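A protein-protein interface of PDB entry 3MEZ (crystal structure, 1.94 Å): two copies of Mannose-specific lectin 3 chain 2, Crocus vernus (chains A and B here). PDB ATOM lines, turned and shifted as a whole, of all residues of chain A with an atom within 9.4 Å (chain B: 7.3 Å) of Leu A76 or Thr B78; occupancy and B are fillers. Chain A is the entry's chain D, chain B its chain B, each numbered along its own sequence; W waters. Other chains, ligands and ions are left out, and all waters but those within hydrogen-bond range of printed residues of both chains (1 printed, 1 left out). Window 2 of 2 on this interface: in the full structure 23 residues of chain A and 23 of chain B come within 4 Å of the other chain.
Water W1 bridges O of His A58 and NH2 of Arg B62.
Phe A60 touches Arg B62, and with the chains exchanged Arg A62 touches Phe B60.
Asp A70 touches Leu B76, and with the chains exchanged Leu A76 touches Asp B70.
Thr A72 touches Leu B76, and with the chains exchanged Leu A76 touches Thr B72.
Leu A76 touches Thr B78, and with the chains exchanged Thr A78 touches Leu B76.
Of the 11 pairs that touch across the chains among the printed residues, 8 have their exchanged pair printed and touching as well.
NH2 of Arg B62 is in salt-bridge range of OD1 of Asp A74.
The side-chain carboxylate (OD2) of Asp A74 lies close to the side-chain carboxylate (OE1) of Glu B68, 3.3 Å away.
Printed residues of chain B that touch a printed residue of chain A: Phe B60, Arg B62, Glu B68, Asp B70, Thr B72, Leu B76 and Thr B78.
Along chain B the printed residues that touch a printed residue of chain A span positions 60 to 78.
Among the printed residues, Asp or Glu carboxylates within 4 Å of a Lys or Arg side-chain nitrogen of the other chain: Asp A74 with Arg B62 (2.8 Å).
NH2 of Arg B62 touches O of His A58 (3.7 Å).
Arg B62 touches Phe A60.
NE of Arg A62 touches CE1 of Phe B60 (3.4 Å).
Asp A70 touches Leu B76 (OD2 to CD1, 3.5 Å).
Thr A72 touches Leu B76 (CG2 to CD1, 3.9 Å).
Asp B70 touches Leu A76.
Leu A76 touches Thr B72 (CD1 to OG1, 3.4 Å).
Leu A76 touches Thr B78 (CD1 to CG2, 3.3 Å).
CD1 of Leu B76 touches OG1 of Thr A78 (3.5 Å).
O of Phe B60 sits at hydrogen-bond distance from N of Thr B72, 2.8 Å away.
The backbone NH (N) of Arg B62 sits at hydrogen-bond distance from the backbone carbonyl oxygen (O) of Asp B70, at 3.1 Å.
OD1 of Asp B73 is in hydrogen-bond range of N of Leu B76 (3.1 Å).
O of Phe A60 lies within hydrogen-bond range of N of Thr A72, 2.8 Å away.
The backbone NH (N) of Arg A62 is in hydrogen-bond range of the backbone carbonyl oxygen (O) of Asp A70 (3.0 Å).
N of Leu A76 sits at hydrogen-bond distance from OD1 of Asp A73, at 3.3 Å.
Leu A76 touches just these residues of chain B: Asp B70, Thr B72 and Thr B78.
Of chain A, only Leu A76 (3.3 Å) comes within 4 Å of Thr B78.
Of the printed residues of chain A, Glu B68 touches Asp A74 (3.3 Å).
Printed residues of chain B within 4 Å of Thr A72: Leu B76.
Printed residues of chain B within 4 Å of Thr A78: Leu B76.
Of the printed residues of chain B, Phe A60 touches Arg B62.
Arg B75 touches none of the printed residues of chain A.
Ile A71 touches none of the printed residues of chain B.
The nearest residue of chain B that does not touch Leu A76 is Arg B62 (4.4 Å).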
ATOM      1  N   VAL A  14     -19.626 -22.322   5.241  1.00  0.00           N
ATOM      2  CA  VAL A  14     -20.049 -23.374   6.089  1.00  0.00           C
ATOM      3  C   VAL A  14     -21.366 -24.020   5.583  1.00  0.00           C
ATOM      4  O   VAL A  14     -22.151 -23.383   4.989  1.00  0.00           O
ATOM      5  CB  VAL A  14     -20.219 -22.707   7.451  1.00  0.00           C
ATOM      6  CG1 VAL A  14     -21.625 -22.706   7.931  1.00  0.00           C
ATOM      7  CG2 VAL A  14     -19.251 -23.143   8.364  1.00  0.00           C
ATOM      8  N   HIS A  58     -25.249 -31.525  15.655  1.00  0.00           N
ATOM      9  CA  HIS A  58     -25.154 -30.183  15.115  1.00  0.00           C
ATOM     10  C   HIS A  58     -23.840 -29.930  14.354  1.00  0.00           C
ATOM     11  O   HIS A  58     -23.252 -28.922  14.509  1.00  0.00           O
ATOM     12  CB  HIS A  58     -25.335 -29.176  16.235  1.00  0.00           C
ATOM     13  CG  HIS A  58     -26.551 -29.410  17.055  1.00  0.00           C
ATOM     14  ND1 HIS A  58     -26.500 -29.937  18.316  1.00  0.00           N
ATOM     15  CD2 HIS A  58     -27.851 -29.214  16.784  1.00  0.00           C
ATOM     16  CE1 HIS A  58     -27.713 -30.053  18.792  1.00  0.00           C
ATOM     17  NE2 HIS A  58     -28.555 -29.630  17.878  1.00  0.00           N
ATOM     18  N   CYS A  59     -23.392 -30.906  13.587  1.00  0.00           N
ATOM     19  CA  CYS A  59     -22.187 -30.811  12.825  1.00  0.00           C
ATOM     20  C   CYS A  59     -22.291 -29.793  11.680  1.00  0.00           C
ATOM     21  O   CYS A  59     -23.338 -29.532  11.177  1.00  0.00           O
ATOM     22  CB  CYS A  59     -21.770 -32.187  12.280  1.00  0.00           C
ATOM     23  SG  CYS A  59     -21.414 -33.386  13.541  1.00  0.00           S
ATOM     24  N   PHE A  60     -21.162 -29.223  11.328  1.00  0.00           N
ATOM     25  CA  PHE A  60     -21.070 -28.405  10.181  1.00  0.00           C
ATOM     26  C   PHE A  60     -19.846 -28.754   9.347  1.00  0.00           C
ATOM     27  O   PHE A  60     -18.913 -29.224   9.867  1.00  0.00           O
ATOM     28  CB  PHE A  60     -21.107 -26.922  10.542  1.00  0.00           C
ATOM     29  CG  PHE A  60     -19.938 -26.413  11.348  1.00  0.00           C
ATOM     30  CD1 PHE A  60     -18.952 -25.686  10.777  1.00  0.00           C
ATOM     31  CD2 PHE A  60     -19.900 -26.558  12.697  1.00  0.00           C
ATOM     32  CE1 PHE A  60     -17.934 -25.163  11.517  1.00  0.00           C
ATOM     33  CE2 PHE A  60     -18.870 -26.026  13.431  1.00  0.00           C
ATOM     34  CZ  PHE A  60     -17.905 -25.342  12.837  1.00  0.00           C
ATOM     35  N   ARG A  62     -16.910 -27.067   6.870  1.00  0.00           N
ATOM     36  CA  ARG A  62     -16.262 -25.821   6.556  1.00  0.00           C
ATOM     37  C   ARG A  62     -15.053 -25.994   5.637  1.00  0.00           C
ATOM     38  O   ARG A  62     -14.277 -26.863   5.849  1.00  0.00           O
ATOM     39  CB  ARG A  62     -15.859 -25.072   7.838  1.00  0.00           C
ATOM     40  CG  ARG A  62     -15.117 -23.769   7.608  1.00  0.00           C
ATOM     41  CD  ARG A  62     -14.628 -23.145   8.898  1.00  0.00           C
ATOM     42  NE  ARG A  62     -13.921 -21.899   8.764  1.00  0.00           N
ATOM     43  CZ  ARG A  62     -12.626 -21.811   8.575  1.00  0.00           C
ATOM     44  NH1 ARG A  62     -11.908 -22.893   8.488  1.00  0.00           N
ATOM     45  NH2 ARG A  62     -12.056 -20.657   8.465  1.00  0.00           N
ATOM     46  N   ASP A  70     -13.177 -29.606   6.637  1.00  0.00           N
ATOM     47  CA  ASP A  70     -13.396 -30.179   7.946  1.00  0.00           C
ATOM     48  C   ASP A  70     -14.886 -30.408   8.215  1.00  0.00           C
ATOM     49  O   ASP A  70     -15.680 -29.583   7.908  1.00  0.00           O
ATOM     50  CB  ASP A  70     -12.901 -29.231   9.014  1.00  0.00           C
ATOM     51  CG  ASP A  70     -11.422 -28.984   8.968  1.00  0.00           C
ATOM     52  OD1 ASP A  70     -10.664 -29.910   8.913  1.00  0.00           O
ATOM     53  OD2 ASP A  70     -11.046 -27.849   9.023  1.00  0.00           O
ATOM     54  N   ILE A  71     -15.243 -31.519   8.818  1.00  0.00           N
ATOM     55  CA  ILE A  71     -16.529 -31.672   9.387  1.00  0.00           C
ATOM     56  C   ILE A  71     -16.340 -31.509  10.891  1.00  0.00           C
ATOM     57  O   ILE A  71     -15.502 -32.148  11.471  1.00  0.00           O
ATOM     58  CB  ILE A  71     -17.168 -33.025   9.089  1.00  0.00           C
ATOM     59  CG1 ILE A  71     -17.358 -33.189   7.589  1.00  0.00           C
ATOM     60  CG2 ILE A  71     -18.453 -33.118   9.784  1.00  0.00           C
ATOM     61  CD1 ILE A  71     -17.846 -34.506   7.150  1.00  0.00           C
ATOM     62  N   THR A  72     -17.103 -30.621  11.496  1.00  0.00           N
ATOM     63  CA  THR A  72     -16.943 -30.347  12.892  1.00  0.00           C
ATOM     64  C   THR A  72     -18.209 -30.314  13.717  1.00  0.00           C
ATOM     65  O   THR A  72     -19.214 -29.922  13.259  1.00  0.00           O
ATOM     66  CB  THR A  72     -16.000 -29.165  13.148  1.00  0.00           C
ATOM     67  OG1 THR A  72     -16.575 -28.242  14.027  1.00  0.00           O
ATOM     68  CG2 THR A  72     -15.484 -28.490  11.892  1.00  0.00           C
ATOM     69  N   ASP A  73     -18.115 -30.797  14.932  1.00  0.00           N
ATOM     70  CA  ASP A  73     -19.227 -30.815  15.855  1.00  0.00           C
ATOM     71  C   ASP A  73     -19.403 -29.558  16.686  1.00  0.00           C
ATOM     72  O   ASP A  73     -18.637 -28.652  16.600  1.00  0.00           O
ATOM     73  CB  ASP A  73     -19.243 -32.065  16.699  1.00  0.00           C
ATOM     74  CG  ASP A  73     -18.156 -32.097  17.713  1.00  0.00           C
ATOM     75  OD1 ASP A  73     -17.622 -31.079  18.059  1.00  0.00           O
ATOM     76  OD2 ASP A  73     -17.829 -33.197  18.131  1.00  0.00           O
ATOM     77  N   ASP A  74     -20.434 -29.548  17.506  1.00  0.00           N
ATOM     78  CA  ASP A  74     -20.829 -28.357  18.247  1.00  0.00           C
ATOM     79  C   ASP A  74     -19.747 -27.890  19.200  1.00  0.00           C
ATOM     80  O   ASP A  74     -19.657 -26.751  19.504  1.00  0.00           O
ATOM     81  CB  ASP A  74     -22.141 -28.559  18.970  1.00  0.00           C
ATOM     82  CG  ASP A  74     -22.735 -27.253  19.492  1.00  0.00           C
ATOM     83  OD1 ASP A  74     -22.974 -26.365  18.697  1.00  0.00           O
ATOM     84  OD2 ASP A  74     -22.966 -27.161  20.673  1.00  0.00           O
ATOM     85  N   ARG A  75     -18.926 -28.815  19.634  1.00  0.00           N
ATOM     86  CA  ARG A  75     -17.873 -28.591  20.596  1.00  0.00           C
ATOM     87  C   ARG A  75     -16.603 -28.126  19.921  1.00  0.00           C
ATOM     88  O   ARG A  75     -15.611 -27.902  20.540  1.00  0.00           O
ATOM     89  CB  ARG A  75     -17.633 -29.867  21.399  1.00  0.00           C
ATOM     90  CG  ARG A  75     -18.764 -30.219  22.299  1.00  0.00           C
ATOM     91  CD  ARG A  75     -18.538 -31.535  23.033  1.00  0.00           C
ATOM     92  NE  ARG A  75     -18.919 -32.679  22.238  1.00  0.00           N
ATOM     93  CZ  ARG A  75     -20.165 -32.935  21.847  1.00  0.00           C
ATOM     94  NH1 ARG A  75     -21.152 -32.129  22.201  1.00  0.00           N
ATOM     95  NH2 ARG A  75     -20.426 -33.993  21.094  1.00  0.00           N
ATOM     96  N   LEU A  76     -16.687 -27.992  18.616  1.00  0.00           N
ATOM     97  CA  LEU A  76     -15.616 -27.589  17.777  1.00  0.00           C
ATOM     98  C   LEU A  76     -14.534 -28.665  17.616  1.00  0.00           C
ATOM     99  O   LEU A  76     -13.435 -28.380  17.273  1.00  0.00           O
ATOM    100  CB  LEU A  76     -15.027 -26.261  18.207  1.00  0.00           C
ATOM    101  CG  LEU A  76     -15.900 -25.000  18.118  1.00  0.00           C
ATOM    102  CD1 LEU A  76     -15.092 -23.784  18.305  1.00  0.00           C
ATOM    103  CD2 LEU A  76     -16.652 -24.910  16.840  1.00  0.00           C
ATOM    104  N   ASN A  77     -14.879 -29.905  17.855  1.00  0.00           N
ATOM    105  CA  ASN A  77     -13.983 -30.993  17.543  1.00  0.00           C
ATOM    106  C   ASN A  77     -14.154 -31.469  16.115  1.00  0.00           C
ATOM    107  O   ASN A  77     -15.218 -31.531  15.646  1.00  0.00           O
ATOM    108  CB  ASN A  77     -14.171 -32.145  18.501  1.00  0.00           C
ATOM    109  CG  ASN A  77     -13.850 -31.787  19.909  1.00  0.00           C
ATOM    110  OD1 ASN A  77     -12.978 -30.993  20.183  1.00  0.00           O
ATOM    111  ND2 ASN A  77     -14.569 -32.374  20.807  1.00  0.00           N
ATOM    112  N   THR A  78     -13.079 -31.787  15.442  1.00  0.00           N
ATOM    113  CA  THR A  78     -13.156 -32.304  14.108  1.00  0.00           C
ATOM    114  C   THR A  78     -13.527 -33.787  14.038  1.00  0.00           C
ATOM    115  O   THR A  78     -12.903 -34.613  14.644  1.00  0.00           O
ATOM    116  CB  THR A  78     -11.837 -32.104  13.416  1.00  0.00           C
ATOM    117  OG1 THR A  78     -11.584 -30.719  13.272  1.00  0.00           O
ATOM    118  CG2 THR A  78     -11.896 -32.685  12.101  1.00  0.00           C
ATOM    119  N   VAL A  79     -14.560 -34.119  13.296  1.00  0.00           N
ATOM    120  CA  VAL A  79     -14.883 -35.506  13.080  1.00  0.00           C
ATOM    121  C   VAL A  79     -14.430 -36.111  11.737  1.00  0.00           C
ATOM    122  O   VAL A  79     -14.414 -37.275  11.595  1.00  0.00           O
ATOM    123  CB  VAL A  79     -16.353 -35.821  13.364  1.00  0.00           C
ATOM    124  CG1 VAL A  79     -16.773 -35.217  14.680  1.00  0.00           C
ATOM    125  CG2 VAL A  79     -17.244 -35.336  12.273  1.00  0.00           C
ATOM    126  N   VAL A  81     -11.514 -34.772   8.459  1.00  0.00           N
ATOM    127  CA  VAL A  81     -10.817 -33.794   7.659  1.00  0.00           C
ATOM    128  C   VAL A  81     -10.145 -34.358   6.397  1.00  0.00           C
ATOM    129  O   VAL A  81      -9.655 -35.449   6.403  1.00  0.00           O
ATOM    130  CB  VAL A  81      -9.736 -33.125   8.415  1.00  0.00           C
ATOM    131  CG1 VAL A  81      -9.220 -32.009   7.637  1.00  0.00           C
ATOM    132  CG2 VAL A  81     -10.230 -32.688   9.713  1.00  0.00           C
ATOM    133  N   ARG B  55      -5.331 -11.859  16.600  1.00  0.00           N
ATOM    134  CA  ARG B  55      -5.329 -13.285  16.808  1.00  0.00           C
ATOM    135  C   ARG B  55      -5.488 -14.156  15.566  1.00  0.00           C
ATOM    136  O   ARG B  55      -5.311 -15.338  15.640  1.00  0.00           O
ATOM    137  CB  ARG B  55      -6.331 -13.687  17.878  1.00  0.00           C
ATOM    138  CG  ARG B  55      -5.910 -13.360  19.265  1.00  0.00           C
ATOM    139  CD  ARG B  55      -5.245 -14.528  19.954  1.00  0.00           C
ATOM    140  NE  ARG B  55      -5.003 -14.304  21.371  1.00  0.00           N
ATOM    141  CZ  ARG B  55      -4.893 -15.262  22.298  1.00  0.00           C
ATOM    142  NH1 ARG B  55      -4.987 -16.545  21.977  1.00  0.00           N
ATOM    143  NH2 ARG B  55      -4.661 -14.927  23.568  1.00  0.00           N
ATOM    144  N   PHE B  60     -13.672 -16.600  12.649  1.00  0.00           N
ATOM    145  CA  PHE B  60     -15.111 -16.605  12.585  1.00  0.00           C
ATOM    146  C   PHE B  60     -15.742 -16.738  13.956  1.00  0.00           C
ATOM    147  O   PHE B  60     -15.206 -17.360  14.810  1.00  0.00           O
ATOM    148  CB  PHE B  60     -15.673 -17.653  11.603  1.00  0.00           C
ATOM    149  CG  PHE B  60     -15.497 -19.080  12.010  1.00  0.00           C
ATOM    150  CD1 PHE B  60     -14.338 -19.741  11.723  1.00  0.00           C
ATOM    151  CD2 PHE B  60     -16.502 -19.777  12.608  1.00  0.00           C
ATOM    152  CE1 PHE B  60     -14.175 -21.019  12.041  1.00  0.00           C
ATOM    153  CE2 PHE B  60     -16.332 -21.062  12.933  1.00  0.00           C
ATOM    154  CZ  PHE B  60     -15.148 -21.693  12.642  1.00  0.00           C
ATOM    155  N   ARG B  62     -19.227 -18.069  15.970  1.00  0.00           N
ATOM    156  CA  ARG B  62     -20.275 -19.034  15.871  1.00  0.00           C
ATOM    157  C   ARG B  62     -21.055 -19.142  17.162  1.00  0.00           C
ATOM    158  O   ARG B  62     -20.493 -19.258  18.189  1.00  0.00           O
ATOM    159  CB  ARG B  62     -19.714 -20.415  15.493  1.00  0.00           C
ATOM    160  CG  ARG B  62     -20.717 -21.539  15.487  1.00  0.00           C
ATOM    161  CD  ARG B  62     -20.141 -22.918  15.115  1.00  0.00           C
ATOM    162  NE  ARG B  62     -21.093 -24.017  15.107  1.00  0.00           N
ATOM    163  CZ  ARG B  62     -21.477 -24.704  16.172  1.00  0.00           C
ATOM    164  NH1 ARG B  62     -21.001 -24.422  17.339  1.00  0.00           N
ATOM    165  NH2 ARG B  62     -22.323 -25.681  16.074  1.00  0.00           N
ATOM    166  N   GLU B  68     -23.175 -21.064  23.724  1.00  0.00           N
ATOM    167  CA  GLU B  68     -21.822 -20.537  23.720  1.00  0.00           C
ATOM    168  C   GLU B  68     -21.492 -19.718  22.486  1.00  0.00           C
ATOM    169  O   GLU B  68     -21.879 -20.089  21.450  1.00  0.00           O
ATOM    170  CB  GLU B  68     -20.797 -21.682  23.899  1.00  0.00           C
ATOM    171  CG  GLU B  68     -20.431 -22.506  22.669  1.00  0.00           C
ATOM    172  CD  GLU B  68     -21.439 -23.583  22.309  1.00  0.00           C
ATOM    173  OE1 GLU B  68     -21.084 -24.657  21.836  1.00  0.00           O
ATOM    174  OE2 GLU B  68     -22.599 -23.348  22.467  1.00  0.00           O
ATOM    175  N   ASP B  70     -18.202 -18.730  20.377  1.00  0.00           N
ATOM    176  CA  ASP B  70     -16.799 -18.979  20.117  1.00  0.00           C
ATOM    177  C   ASP B  70     -16.274 -18.123  18.977  1.00  0.00           C
ATOM    178  O   ASP B  70     -16.915 -18.005  17.994  1.00  0.00           O
ATOM    179  CB  ASP B  70     -16.558 -20.448  19.734  1.00  0.00           C
ATOM    180  CG  ASP B  70     -17.073 -21.430  20.758  1.00  0.00           C
ATOM    181  OD1 ASP B  70     -16.692 -21.331  21.891  1.00  0.00           O
ATOM    182  OD2 ASP B  70     -17.864 -22.287  20.428  1.00  0.00           O
ATOM    183  N   ILE B  71     -15.107 -17.541  19.152  1.00  0.00           N
ATOM    184  CA  ILE B  71     -14.341 -16.992  18.084  1.00  0.00           C
ATOM    185  C   ILE B  71     -13.221 -17.974  17.745  1.00  0.00           C
ATOM    186  O   ILE B  71     -12.412 -18.304  18.556  1.00  0.00           O
ATOM    187  CB  ILE B  71     -13.734 -15.633  18.396  1.00  0.00           C
ATOM    188  CG1 ILE B  71     -14.802 -14.658  18.810  1.00  0.00           C
ATOM    189  CG2 ILE B  71     -13.044 -15.129  17.242  1.00  0.00           C
ATOM    190  CD1 ILE B  71     -14.305 -13.387  19.263  1.00  0.00           C
ATOM    191  N   THR B  72     -13.225 -18.415  16.504  1.00  0.00           N
ATOM    192  CA  THR B  72     -12.465 -19.527  16.030  1.00  0.00           C
ATOM    193  C   THR B  72     -11.569 -19.129  14.882  1.00  0.00           C
ATOM    194  O   THR B  72     -11.967 -18.400  14.049  1.00  0.00           O
ATOM    195  CB  THR B  72     -13.429 -20.635  15.563  1.00  0.00           C
ATOM    196  OG1 THR B  72     -14.381 -20.916  16.585  1.00  0.00           O
ATOM    197  CG2 THR B  72     -12.697 -21.869  15.230  1.00  0.00           C
ATOM    198  N   ASP B  73     -10.347 -19.591  14.888  1.00  0.00           N
ATOM    199  CA  ASP B  73      -9.438 -19.362  13.783  1.00  0.00           C
ATOM    200  C   ASP B  73      -9.514 -20.400  12.658  1.00  0.00           C
ATOM    201  O   ASP B  73     -10.183 -21.364  12.778  1.00  0.00           O
ATOM    202  CB  ASP B  73      -8.007 -19.118  14.253  1.00  0.00           C
ATOM    203  CG  ASP B  73      -7.314 -20.366  14.734  1.00  0.00           C
ATOM    204  OD1 ASP B  73      -7.788 -21.451  14.607  1.00  0.00           O
ATOM    205  OD2 ASP B  73      -6.276 -20.202  15.305  1.00  0.00           O
ATOM    206  N   ARG B  75      -7.618 -22.683  11.877  1.00  0.00           N
ATOM    207  CA  ARG B  75      -7.145 -23.977  12.306  1.00  0.00           C
ATOM    208  C   ARG B  75      -8.128 -24.637  13.236  1.00  0.00           C
ATOM    209  O   ARG B  75      -7.899 -25.679  13.720  1.00  0.00           O
ATOM    210  CB  ARG B  75      -5.768 -23.867  12.949  1.00  0.00           C
ATOM    211  CG  ARG B  75      -4.715 -23.351  12.025  1.00  0.00           C
ATOM    212  CD  ARG B  75      -3.421 -23.102  12.713  1.00  0.00           C
ATOM    213  NE  ARG B  75      -3.280 -23.967  13.864  1.00  0.00           N
ATOM    214  CZ  ARG B  75      -2.957 -25.257  13.828  1.00  0.00           C
ATOM    215  NH1 ARG B  75      -2.729 -25.857  12.680  1.00  0.00           N
ATOM    216  NH2 ARG B  75      -2.880 -25.948  14.961  1.00  0.00           N
ATOM    217  N   LEU B  76      -9.229 -23.973  13.470  1.00  0.00           N
ATOM    218  CA  LEU B  76     -10.265 -24.401  14.364  1.00  0.00           C
ATOM    219  C   LEU B  76      -9.929 -24.290  15.854  1.00  0.00           C
ATOM    220  O   LEU B  76     -10.586 -24.881  16.652  1.00  0.00           O
ATOM    221  CB  LEU B  76     -10.790 -25.778  14.010  1.00  0.00           C
ATOM    222  CG  LEU B  76     -11.408 -25.954  12.630  1.00  0.00           C
ATOM    223  CD1 LEU B  76     -11.839 -27.341  12.422  1.00  0.00           C
ATOM    224  CD2 LEU B  76     -12.556 -25.055  12.426  1.00  0.00           C
ATOM    225  N   ASN B  77      -8.908 -23.533  16.210  1.00  0.00           N
ATOM    226  CA  ASN B  77      -8.637 -23.251  17.612  1.00  0.00           C
ATOM    227  C   ASN B  77      -9.534 -22.097  18.070  1.00  0.00           C
ATOM    228  O   ASN B  77      -9.719 -21.160  17.359  1.00  0.00           O
ATOM    229  CB  ASN B  77      -7.181 -22.856  17.884  1.00  0.00           C
ATOM    230  CG  ASN B  77      -6.148 -23.861  17.364  1.00  0.00           C
ATOM    231  OD1 ASN B  77      -6.234 -25.034  17.607  1.00  0.00           O
ATOM    232  ND2 ASN B  77      -5.151 -23.351  16.685  1.00  0.00           N
ATOM    233  N   THR B  78     -10.055 -22.180  19.280  1.00  0.00           N
ATOM    234  CA  THR B  78     -10.886 -21.130  19.784  1.00  0.00           C
ATOM    235  C   THR B  78     -10.040 -20.070  20.452  1.00  0.00           C
ATOM    236  O   THR B  78      -9.359 -20.314  21.373  1.00  0.00           O
ATOM    237  CB  THR B  78     -11.919 -21.654  20.742  1.00  0.00           C
ATOM    238  OG1 THR B  78     -11.278 -22.059  21.932  1.00  0.00           O
ATOM    239  CG2 THR B  78     -12.548 -22.823  20.210  1.00  0.00           C
ATOM    240  N   VAL B  79     -10.061 -18.911  19.866  1.00  0.00           N
ATOM    241  CA  VAL B  79      -9.520 -17.656  20.336  1.00  0.00           C
ATOM    242  C   VAL B  79     -10.224 -17.002  21.547  1.00  0.00           C
ATOM    243  O   VAL B  79      -9.612 -16.304  22.316  1.00  0.00           O
ATOM    244  CB  VAL B  79      -9.419 -16.730  19.154  1.00  0.00           C
ATOM    245  CG1 VAL B  79      -9.092 -15.411  19.522  1.00  0.00           C
ATOM    246  CG2 VAL B  79      -8.332 -17.228  18.258  1.00  0.00           C
ATOM    247  N   PHE B  80     -11.534 -17.147  21.627  1.00  0.00           N
ATOM    248  CA  PHE B  80     -12.339 -16.580  22.699  1.00  0.00           C
ATOM    249  C   PHE B  80     -13.577 -17.422  22.862  1.00  0.00           C
ATOM    250  O   PHE B  80     -14.134 -17.811  21.907  1.00  0.00           O
ATOM    251  CB  PHE B  80     -12.717 -15.144  22.335  1.00  0.00           C
ATOM    252  CG  PHE B  80     -13.855 -14.576  23.109  1.00  0.00           C
ATOM    253  CD1 PHE B  80     -13.628 -13.725  24.151  1.00  0.00           C
ATOM    254  CD2 PHE B  80     -15.144 -14.862  22.789  1.00  0.00           C
ATOM    255  CE1 PHE B  80     -14.681 -13.199  24.857  1.00  0.00           C
ATOM    256  CE2 PHE B  80     -16.162 -14.344  23.483  1.00  0.00           C
ATOM    257  CZ  PHE B  80     -15.934 -13.505  24.509  1.00  0.00           C
ATOM    258  N   VAL B  81     -14.009 -17.692  24.072  1.00  0.00           N
ATOM    259  CA  VAL B  81     -15.297 -18.267  24.259  1.00  0.00           C
ATOM    260  C   VAL B  81     -16.031 -17.594  25.408  1.00  0.00           C
ATOM    261  O   VAL B  81     -15.438 -17.206  26.376  1.00  0.00           O
ATOM    262  CB  VAL B  81     -15.244 -19.755  24.516  1.00  0.00           C
ATOM    263  CG1 VAL B  81     -16.583 -20.316  24.469  1.00  0.00           C
ATOM    264  CG2 VAL B  81     -14.427 -20.429  23.530  1.00  0.00           C
HETATM  265  O   HOH W   1     -23.717 -26.446  13.244  1.00  0.00           O
